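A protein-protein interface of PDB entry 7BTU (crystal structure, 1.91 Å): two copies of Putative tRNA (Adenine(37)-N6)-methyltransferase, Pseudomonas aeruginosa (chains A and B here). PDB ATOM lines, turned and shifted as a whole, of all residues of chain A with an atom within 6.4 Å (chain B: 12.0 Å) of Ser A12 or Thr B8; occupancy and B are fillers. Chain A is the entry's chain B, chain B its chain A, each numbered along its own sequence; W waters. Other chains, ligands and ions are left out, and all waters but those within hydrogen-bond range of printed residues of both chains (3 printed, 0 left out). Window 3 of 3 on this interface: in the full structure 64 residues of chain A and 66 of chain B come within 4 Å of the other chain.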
ATOM      1  N   SER A  10     -13.924  27.774  17.060  1.00  0.00           N
ATOM      2  CA  SER A  10     -14.776  26.832  16.339  1.00  0.00           C
ATOM      3  C   SER A  10     -14.193  26.558  14.960  1.00  0.00           C
ATOM      4  O   SER A  10     -13.792  27.494  14.253  1.00  0.00           O
ATOM      5  CB  SER A  10     -16.210  27.373  16.232  1.00  0.00           C
ATOM      6  OG  SER A  10     -17.047  26.365  15.671  1.00  0.00           O
ATOM      7  N   VAL A  11     -14.123  25.275  14.577  1.00  0.00           N
ATOM      8  CA  VAL A  11     -13.710  24.927  13.218  1.00  0.00           C
ATOM      9  C   VAL A  11     -14.835  24.134  12.561  1.00  0.00           C
ATOM     10  O   VAL A  11     -15.669  23.500  13.233  1.00  0.00           O
ATOM     11  CB  VAL A  11     -12.370  24.135  13.189  1.00  0.00           C
ATOM     12  CG1 VAL A  11     -11.259  24.987  13.830  1.00  0.00           C
ATOM     13  CG2 VAL A  11     -12.519  22.782  13.888  1.00  0.00           C
ATOM     14  N   SER A  12     -14.836  24.140  11.228  1.00  0.00           N
ATOM     15  CA  SER A  12     -15.821  23.385  10.445  1.00  0.00           C
ATOM     16  C   SER A  12     -15.143  22.760   9.235  1.00  0.00           C
ATOM     17  O   SER A  12     -14.228  23.365   8.666  1.00  0.00           O
ATOM     18  CB  SER A  12     -16.943  24.307   9.928  1.00  0.00           C
ATOM     19  OG  SER A  12     -17.905  24.529  10.908  1.00  0.00           O
ATOM     20  N   PRO A  13     -15.568  21.572   8.808  1.00  0.00           N
ATOM     21  CA  PRO A  13     -14.865  20.927   7.689  1.00  0.00           C
ATOM     22  C   PRO A  13     -14.992  21.779   6.441  1.00  0.00           C
ATOM     23  O   PRO A  13     -16.052  22.341   6.174  1.00  0.00           O
ATOM     24  CB  PRO A  13     -15.588  19.584   7.504  1.00  0.00           C
ATOM     25  CG  PRO A  13     -16.515  19.414   8.732  1.00  0.00           C
ATOM     26  CD  PRO A  13     -16.685  20.784   9.367  1.00  0.00           C
ATOM     27  N   ILE A  14     -13.897  21.848   5.666  1.00  0.00           N
ATOM     28  CA  ILE A  14     -13.978  22.352   4.293  1.00  0.00           C
ATOM     29  C   ILE A  14     -14.386  21.260   3.317  1.00  0.00           C
ATOM     30  O   ILE A  14     -14.699  21.555   2.164  1.00  0.00           O
ATOM     31  CB  ILE A  14     -12.620  22.961   3.918  1.00  0.00           C
ATOM     32  CG1 ILE A  14     -11.521  21.935   4.122  1.00  0.00           C
ATOM     33  CG2 ILE A  14     -12.344  24.188   4.838  1.00  0.00           C
ATOM     34  CD1 ILE A  14     -10.241  22.195   3.345  1.00  0.00           C
ATOM     35  N   GLY A  15     -14.378  19.999   3.749  1.00  0.00           N
ATOM     36  CA  GLY A  15     -14.750  18.918   2.844  1.00  0.00           C
ATOM     37  C   GLY A  15     -14.641  17.590   3.578  1.00  0.00           C
ATOM     38  O   GLY A  15     -14.330  17.545   4.777  1.00  0.00           O
ATOM     39  N   PHE A  47     -15.656  26.573  -0.689  1.00  0.00           N
ATOM     40  CA  PHE A  47     -14.338  26.122  -1.116  1.00  0.00           C
ATOM     41  C   PHE A  47     -14.363  25.251  -2.346  1.00  0.00           C
ATOM     42  O   PHE A  47     -13.347  24.590  -2.632  1.00  0.00           O
ATOM     43  CB  PHE A  47     -13.642  25.381   0.027  1.00  0.00           C
ATOM     44  CG  PHE A  47     -13.680  26.165   1.276  1.00  0.00           C
ATOM     45  CD1 PHE A  47     -12.905  27.312   1.390  1.00  0.00           C
ATOM     46  CD2 PHE A  47     -14.572  25.840   2.290  1.00  0.00           C
ATOM     47  CE1 PHE A  47     -12.980  28.107   2.539  1.00  0.00           C
ATOM     48  CE2 PHE A  47     -14.641  26.609   3.421  1.00  0.00           C
ATOM     49  CZ  PHE A  47     -13.843  27.758   3.548  1.00  0.00           C
ATOM     50  N   LEU A  67     -10.223  15.814  11.283  1.00  0.00           N
ATOM     51  CA  LEU A  67     -10.773  15.513  12.591  1.00  0.00           C
ATOM     52  C   LEU A  67     -10.784  14.010  12.790  1.00  0.00           C
ATOM     53  O   LEU A  67     -11.267  13.295  11.902  1.00  0.00           O
ATOM     54  CB  LEU A  67     -12.194  16.041  12.700  1.00  0.00           C
ATOM     55  CG  LEU A  67     -12.339  17.574  12.796  1.00  0.00           C
ATOM     56  CD1 LEU A  67     -13.780  17.961  12.865  1.00  0.00           C
ATOM     57  CD2 LEU A  67     -11.599  18.069  14.025  1.00  0.00           C
ATOM     58  N   VAL A 133     -12.317  17.036   6.746  1.00  0.00           N
ATOM     59  CA  VAL A 133     -11.024  17.702   6.548  1.00  0.00           C
ATOM     60  C   VAL A 133     -11.179  19.180   6.898  1.00  0.00           C
ATOM     61  O   VAL A 133     -12.163  19.813   6.502  1.00  0.00           O
ATOM     62  CB  VAL A 133     -10.531  17.500   5.100  1.00  0.00           C
ATOM     63  CG1 VAL A 133      -9.290  18.373   4.765  1.00  0.00           C
ATOM     64  CG2 VAL A 133     -10.161  15.997   4.894  1.00  0.00           C
ATOM     65  N   LEU A 134     -10.178  19.734   7.603  1.00  0.00           N
ATOM     66  CA  LEU A 134     -10.162  21.152   7.990  1.00  0.00           C
ATOM     67  C   LEU A 134      -9.289  22.033   7.131  1.00  0.00           C
ATOM     68  O   LEU A 134      -9.518  23.274   7.110  1.00  0.00           O
ATOM     69  CB  LEU A 134      -9.656  21.336   9.435  1.00  0.00           C
ATOM     70  CG  LEU A 134     -10.342  20.442  10.457  1.00  0.00           C
ATOM     71  CD1 LEU A 134      -9.663  20.582  11.834  1.00  0.00           C
ATOM     72  CD2 LEU A 134     -11.858  20.857  10.500  1.00  0.00           C
ATOM     73  N   GLU B   3     -28.765  16.944   7.360  1.00  0.00           N
ATOM     74  CA  GLU B   3     -27.912  16.745   6.186  1.00  0.00           C
ATOM     75  C   GLU B   3     -27.235  18.046   5.706  1.00  0.00           C
ATOM     76  O   GLU B   3     -26.152  17.994   5.124  1.00  0.00           O
ATOM     77  CB  GLU B   3     -28.730  16.117   5.045  1.00  0.00           C
ATOM     78  N   PHE B   4     -27.861  19.205   5.978  1.00  0.00           N
ATOM     79  CA  PHE B   4     -27.484  20.475   5.359  1.00  0.00           C
ATOM     80  C   PHE B   4     -27.005  21.528   6.365  1.00  0.00           C
ATOM     81  O   PHE B   4     -26.955  22.726   6.026  1.00  0.00           O
ATOM     82  CB  PHE B   4     -28.658  21.022   4.535  1.00  0.00           C
ATOM     83  CG  PHE B   4     -29.190  20.034   3.531  1.00  0.00           C
ATOM     84  CD1 PHE B   4     -28.470  19.743   2.375  1.00  0.00           C
ATOM     85  CD2 PHE B   4     -30.358  19.361   3.774  1.00  0.00           C
ATOM     86  CE1 PHE B   4     -28.936  18.809   1.462  1.00  0.00           C
ATOM     87  CE2 PHE B   4     -30.858  18.428   2.856  1.00  0.00           C
ATOM     88  CZ  PHE B   4     -30.147  18.152   1.705  1.00  0.00           C
ATOM     89  N   GLU B   5     -26.658  21.100   7.587  1.00  0.00           N
ATOM     90  CA  GLU B   5     -26.109  21.947   8.652  1.00  0.00           C
ATOM     91  C   GLU B   5     -24.622  21.633   8.833  1.00  0.00           C
ATOM     92  O   GLU B   5     -24.268  20.495   9.155  1.00  0.00           O
ATOM     93  CB  GLU B   5     -26.861  21.703   9.968  1.00  0.00           C
ATOM     94  N   LEU B   6     -23.758  22.633   8.640  1.00  0.00           N
ATOM     95  CA  LEU B   6     -22.323  22.389   8.754  1.00  0.00           C
ATOM     96  C   LEU B   6     -21.968  22.009  10.189  1.00  0.00           C
ATOM     97  O   LEU B   6     -22.346  22.701  11.140  1.00  0.00           O
ATOM     98  CB  LEU B   6     -21.502  23.606   8.312  1.00  0.00           C
ATOM     99  N   MET B   7     -21.285  20.871  10.321  1.00  0.00           N
ATOM    100  CA  MET B   7     -20.701  20.408  11.571  1.00  0.00           C
ATOM    101  C   MET B   7     -19.755  21.453  12.156  1.00  0.00           C
ATOM    102  O   MET B   7     -19.025  22.130  11.426  1.00  0.00           O
ATOM    103  CB  MET B   7     -19.951  19.092  11.302  1.00  0.00           C
ATOM    104  CG  MET B   7     -19.106  18.535  12.440  1.00  0.00           C
ATOM    105  SD  MET B   7     -17.686  17.563  11.861  1.00  0.00           S
ATOM    106  CE  MET B   7     -18.465  16.281  10.894  1.00  0.00           C
ATOM    107  N   THR B   8     -19.754  21.581  13.480  1.00  0.00           N
ATOM    108  CA  THR B   8     -18.783  22.429  14.177  1.00  0.00           C
ATOM    109  C   THR B   8     -18.071  21.584  15.222  1.00  0.00           C
ATOM    110  O   THR B   8     -18.600  20.561  15.673  1.00  0.00           O
ATOM    111  CB  THR B   8     -19.450  23.617  14.872  1.00  0.00           C
ATOM    112  OG1 THR B   8     -20.511  23.115  15.716  1.00  0.00           O
ATOM    113  CG2 THR B   8     -20.036  24.556  13.833  1.00  0.00           C
ATOM    114  N   HIS B   9     -16.865  22.010  15.565  1.00  0.00           N
ATOM    115  CA  HIS B   9     -15.991  21.362  16.531  1.00  0.00           C
ATOM    116  C   HIS B   9     -15.224  22.452  17.274  1.00  0.00           C
ATOM    117  O   HIS B   9     -14.561  23.259  16.630  1.00  0.00           O
ATOM    118  CB  HIS B   9     -14.991  20.446  15.782  1.00  0.00           C
ATOM    119  CG  HIS B   9     -13.954  19.818  16.661  1.00  0.00           C
ATOM    120  ND1 HIS B   9     -14.250  18.817  17.562  1.00  0.00           N
ATOM    121  CD2 HIS B   9     -12.627  20.051  16.783  1.00  0.00           C
ATOM    122  CE1 HIS B   9     -13.147  18.440  18.183  1.00  0.00           C
ATOM    123  NE2 HIS B   9     -12.149  19.171  17.729  1.00  0.00           N
ATOM    124  N   SER B  10     -15.264  22.463  18.612  1.00  0.00           N
ATOM    125  CA  SER B  10     -14.520  23.457  19.381  1.00  0.00           C
ATOM    126  C   SER B  10     -13.155  22.923  19.768  1.00  0.00           C
ATOM    127  O   SER B  10     -13.019  21.757  20.164  1.00  0.00           O
ATOM    128  CB  SER B  10     -15.254  23.887  20.657  1.00  0.00           C
ATOM    129  OG  SER B  10     -16.608  24.081  20.342  1.00  0.00           O
ATOM    130  N   VAL B  11     -12.151  23.777  19.630  1.00  0.00           N
ATOM    131  CA  VAL B  11     -10.795  23.502  20.082  1.00  0.00           C
ATOM    132  C   VAL B  11     -10.417  24.573  21.110  1.00  0.00           C
ATOM    133  O   VAL B  11     -10.923  25.708  21.082  1.00  0.00           O
ATOM    134  CB  VAL B  11      -9.783  23.459  18.904  1.00  0.00           C
ATOM    135  CG1 VAL B  11     -10.188  22.364  17.878  1.00  0.00           C
ATOM    136  CG2 VAL B  11      -9.666  24.838  18.252  1.00  0.00           C
ATOM    137  N   SER B  12      -9.504  24.199  22.017  1.00  0.00           N
ATOM    138  CA  SER B  12      -8.994  25.075  23.062  1.00  0.00           C
ATOM    139  C   SER B  12      -7.512  24.785  23.182  1.00  0.00           C
ATOM    140  O   SER B  12      -7.072  23.643  22.973  1.00  0.00           O
ATOM    141  CB  SER B  12      -9.675  24.871  24.439  1.00  0.00           C
ATOM    142  OG  SER B  12     -10.962  25.414  24.447  1.00  0.00           O
ATOM    143  N   LEU B  67      -3.047  28.057  16.671  1.00  0.00           N
ATOM    144  CA  LEU B  67      -4.002  28.998  16.134  1.00  0.00           C
ATOM    145  C   LEU B  67      -3.236  30.207  15.560  1.00  0.00           C
ATOM    146  O   LEU B  67      -2.365  30.757  16.229  1.00  0.00           O
ATOM    147  CB  LEU B  67      -4.970  29.457  17.240  1.00  0.00           C
ATOM    148  CG  LEU B  67      -5.975  28.424  17.752  1.00  0.00           C
ATOM    149  CD1 LEU B  67      -6.823  28.928  18.965  1.00  0.00           C
ATOM    150  CD2 LEU B  67      -6.828  27.923  16.600  1.00  0.00           C
ATOM    151  N   VAL B  93      -5.928  29.729  -1.894  1.00  0.00           N
ATOM    152  CA  VAL B  93      -5.501  29.614  -0.504  1.00  0.00           C
ATOM    153  C   VAL B  93      -4.962  28.218  -0.194  1.00  0.00           C
ATOM    154  O   VAL B  93      -3.993  28.061   0.565  1.00  0.00           O
ATOM    155  CB  VAL B  93      -6.646  29.997   0.442  1.00  0.00           C
ATOM    156  CG1 VAL B  93      -7.837  29.017   0.291  1.00  0.00           C
ATOM    157  CG2 VAL B  93      -6.125  30.052   1.838  1.00  0.00           C
ATOM    158  N   PHE B  94      -5.513  27.200  -0.824  1.00  0.00           N
ATOM    159  CA  PHE B  94      -5.024  25.856  -0.527  1.00  0.00           C
ATOM    160  C   PHE B  94      -3.699  25.521  -1.220  1.00  0.00           C
ATOM    161  O   PHE B  94      -3.097  24.467  -0.941  1.00  0.00           O
ATOM    162  CB  PHE B  94      -6.139  24.865  -0.904  1.00  0.00           C
ATOM    163  CG  PHE B  94      -7.376  25.030  -0.074  1.00  0.00           C
ATOM    164  CD1 PHE B  94      -7.277  25.117   1.288  1.00  0.00           C
ATOM    165  CD2 PHE B  94      -8.618  25.128  -0.663  1.00  0.00           C
ATOM    166  CE1 PHE B  94      -8.432  25.251   2.084  1.00  0.00           C
ATOM    167  CE2 PHE B  94      -9.759  25.286   0.109  1.00  0.00           C
ATOM    168  CZ  PHE B  94      -9.663  25.340   1.491  1.00  0.00           C
ATOM    169  N   ARG B 101      -5.990  31.178   6.861  1.00  0.00           N
ATOM    170  CA  ARG B 101      -6.508  29.887   6.401  1.00  0.00           C
ATOM    171  C   ARG B 101      -7.935  29.742   6.901  1.00  0.00           C
ATOM    172  O   ARG B 101      -8.276  30.240   7.988  1.00  0.00           O
ATOM    173  CB  ARG B 101      -5.677  28.709   6.918  1.00  0.00           C
ATOM    174  CG  ARG B 101      -4.212  28.985   6.868  1.00  0.00           C
ATOM    175  CD  ARG B 101      -3.399  27.786   6.703  1.00  0.00           C
ATOM    176  NE  ARG B 101      -3.754  27.011   5.511  1.00  0.00           N
ATOM    177  CZ  ARG B 101      -3.349  27.281   4.275  1.00  0.00           C
ATOM    178  NH1 ARG B 101      -2.577  28.360   4.011  1.00  0.00           N
ATOM    179  NH2 ARG B 101      -3.750  26.489   3.290  1.00  0.00           N
ATOM    180  N   PRO B 102      -8.785  29.046   6.138  1.00  0.00           N
ATOM    181  CA  PRO B 102     -10.223  28.999   6.474  1.00  0.00           C
ATOM    182  C   PRO B 102     -10.519  28.655   7.928  1.00  0.00           C
ATOM    183  O   PRO B 102     -11.321  29.344   8.557  1.00  0.00           O
ATOM    184  CB  PRO B 102     -10.755  27.941   5.505  1.00  0.00           C
ATOM    185  CG  PRO B 102      -9.867  28.137   4.286  1.00  0.00           C
ATOM    186  CD  PRO B 102      -8.511  28.561   4.773  1.00  0.00           C
ATOM    187  N   ASN B 103      -9.805  27.705   8.514  1.00  0.00           N
ATOM    188  CA  ASN B 103     -10.091  27.334   9.892  1.00  0.00           C
ATOM    189  C   ASN B 103      -9.110  27.898  10.899  1.00  0.00           C
ATOM    190  O   ASN B 103      -9.213  27.574  12.087  1.00  0.00           O
ATOM    191  CB  ASN B 103     -10.146  25.809   9.986  1.00  0.00           C
ATOM    192  CG  ASN B 103     -11.542  25.316   9.670  1.00  0.00           C
ATOM    193  OD1 ASN B 103     -12.510  25.782  10.287  1.00  0.00           O
ATOM    194  ND2 ASN B 103     -11.673  24.436   8.649  1.00  0.00           N
ATOM    195  N   GLY B 104      -8.127  28.670  10.445  1.00  0.00           N
ATOM    196  CA  GLY B 104      -7.272  29.410  11.348  1.00  0.00           C
ATOM    197  C   GLY B 104      -6.278  28.538  12.088  1.00  0.00           C
ATOM    198  O   GLY B 104      -5.765  28.941  13.115  1.00  0.00           O
ATOM    199  N   ILE B 105      -5.993  27.339  11.589  1.00  0.00           N
ATOM    200  CA  ILE B 105      -5.052  26.417  12.241  1.00  0.00           C
ATOM    201  C   ILE B 105      -3.794  26.300  11.404  1.00  0.00           C
ATOM    202  O   ILE B 105      -3.863  25.990  10.207  1.00  0.00           O
ATOM    203  CB  ILE B 105      -5.690  25.039  12.464  1.00  0.00           C
ATOM    204  CG1 ILE B 105      -6.805  25.237  13.471  1.00  0.00           C
ATOM    205  CG2 ILE B 105      -4.639  24.042  13.068  1.00  0.00           C
ATOM    206  CD1 ILE B 105      -7.709  24.014  13.673  1.00  0.00           C
ATOM    207  N   LEU B 134      -2.520  23.947  20.019  1.00  0.00           N
ATOM    208  CA  LEU B 134      -3.588  22.965  20.130  1.00  0.00           C
ATOM    209  C   LEU B 134      -3.085  21.546  20.323  1.00  0.00           C
ATOM    210  O   LEU B 134      -3.801  20.720  20.901  1.00  0.00           O
ATOM    211  CB  LEU B 134      -4.448  22.976  18.855  1.00  0.00           C
ATOM    212  CG  LEU B 134      -5.018  24.348  18.507  1.00  0.00           C
ATOM    213  CD1 LEU B 134      -5.873  24.180  17.283  1.00  0.00           C
ATOM    214  CD2 LEU B 134      -5.892  24.800  19.677  1.00  0.00           C
HETATM  215  O   HOH W   1     -12.816  28.384  11.780  1.00  0.00           O
HETATM  216  O   HOH W   2     -17.615  24.885  18.101  1.00  0.00           O
HETATM  217  O   HOH W   3      -8.218  25.754   6.849  1.00  0.00           O
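Water W2 bridges the side-chain hydroxyl (OG) of Ser B10 and the side-chain hydroxyl (OG) of Ser A10. Water W1 bridges the backbone carbonyl oxygen of Ser A10 (2.8 Å) and the side-chain amide oxygen of Asn B103 (3.0 Å). Water W3 lies within hydrogen-bond range of O of Leu A134 (2.8 Å) and N of Asn B103 (3.0 Å).
Of chain B, only Thr B8 (3.7 Å) and His B9 (3.6 Å) come within 4 Å of Ser A10. Of chain B, only Thr B8 (3.4 Å), His B9 (2.9 Å), Asn B103 (3.3 Å) and Ile B105 (3.7 Å) come within 4 Å of Val A11. Of chain B, only Met B7 (2.7 Å), Thr B8 (3.6 Å) and Asn B103 (2.8 Å) come within 4 Å of Ser A12. Ile A14 touches just these residues of chain B: Phe B94 and Asn B103. Of the printed residues of chain B, Phe A47 touches Phe B94 (3.8 Å) and Pro B102 (3.6 Å). Val A133 touches none of the printed residues of chain B. Of the printed residues of chain B, Leu A134 touches Asn B103. Phe B4 touches none of the printed residues of chain A. Printed residues of chain A within 4 Å of Met B7: Ser A12 and Pro A13. Of the printed residues of chain A, Thr B8 touches Ser A10, Val A11 and Ser A12. Printed residues of chain A within 4 Å of His B9: Ser A10 (3.6 Å), Val A11 (2.9 Å) and Leu A67 (3.5 Å). Of the printed residues of chain A, Pro B102 touches Phe A47. Printed residues of chain A within 4 Å of Ile B105: Val A11. The nearest residue of chain B that does not touch Ser A12 is Leu B6 (4.5 Å).
Printed residues of chain B that touch a printed residue of chain A: Met B7, Thr B8, His B9, Phe B94, Pro B102, Asn B103 and Ile B105. Among the printed residues, no Asp or Glu carboxylate lies within 4 Å of a Lys or Arg side-chain nitrogen of the other chain.
The backbone carbonyl oxygen (O) of Met B7 sits at hydrogen-bond distance from the side-chain hydroxyl (OG) of Ser A12. The backbone carbonyl oxygen (O) of His B9 sits at hydrogen-bond distance from the backbone NH (N) of Val A11 (2.9 Å). ND2 of Asn B103 is in hydrogen-bond range of O of Ser A12, at 2.8 Å. The side-chain amide nitrogen (ND2) of Asn B103 is in hydrogen-bond range of the backbone carbonyl oxygen (O) of Leu A134.
Thr B8 touches Ser A10. Ser A10 touches His B9. CA of Thr B8 touches O of Val A11, at 3.4 Å. Asn B103 touches Val A11. Val A11 touches Ile B105. Ser A12 touches Thr B8 (OG to CG2, 3.6 Å). Asn B103 touches Ile A14 (ND2 to CG2, 3.9 Å). Phe B94 touches Phe A47 (CZ to CD1, 3.8 Å). Phe A47 touches Pro B102. Leu A67 touches His B9 (CD2 to CD2, 3.5 Å).
5 positions are printed for both chains. Of the 16 pairs that touch across the chains among the printed residues, none has its exchanged pair printed and touching as well.
The backbone carbonyl oxygen (O) of Val A133 lies within hydrogen-bond range of the backbone NH (N) of Ile A14 (2.8 Å).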
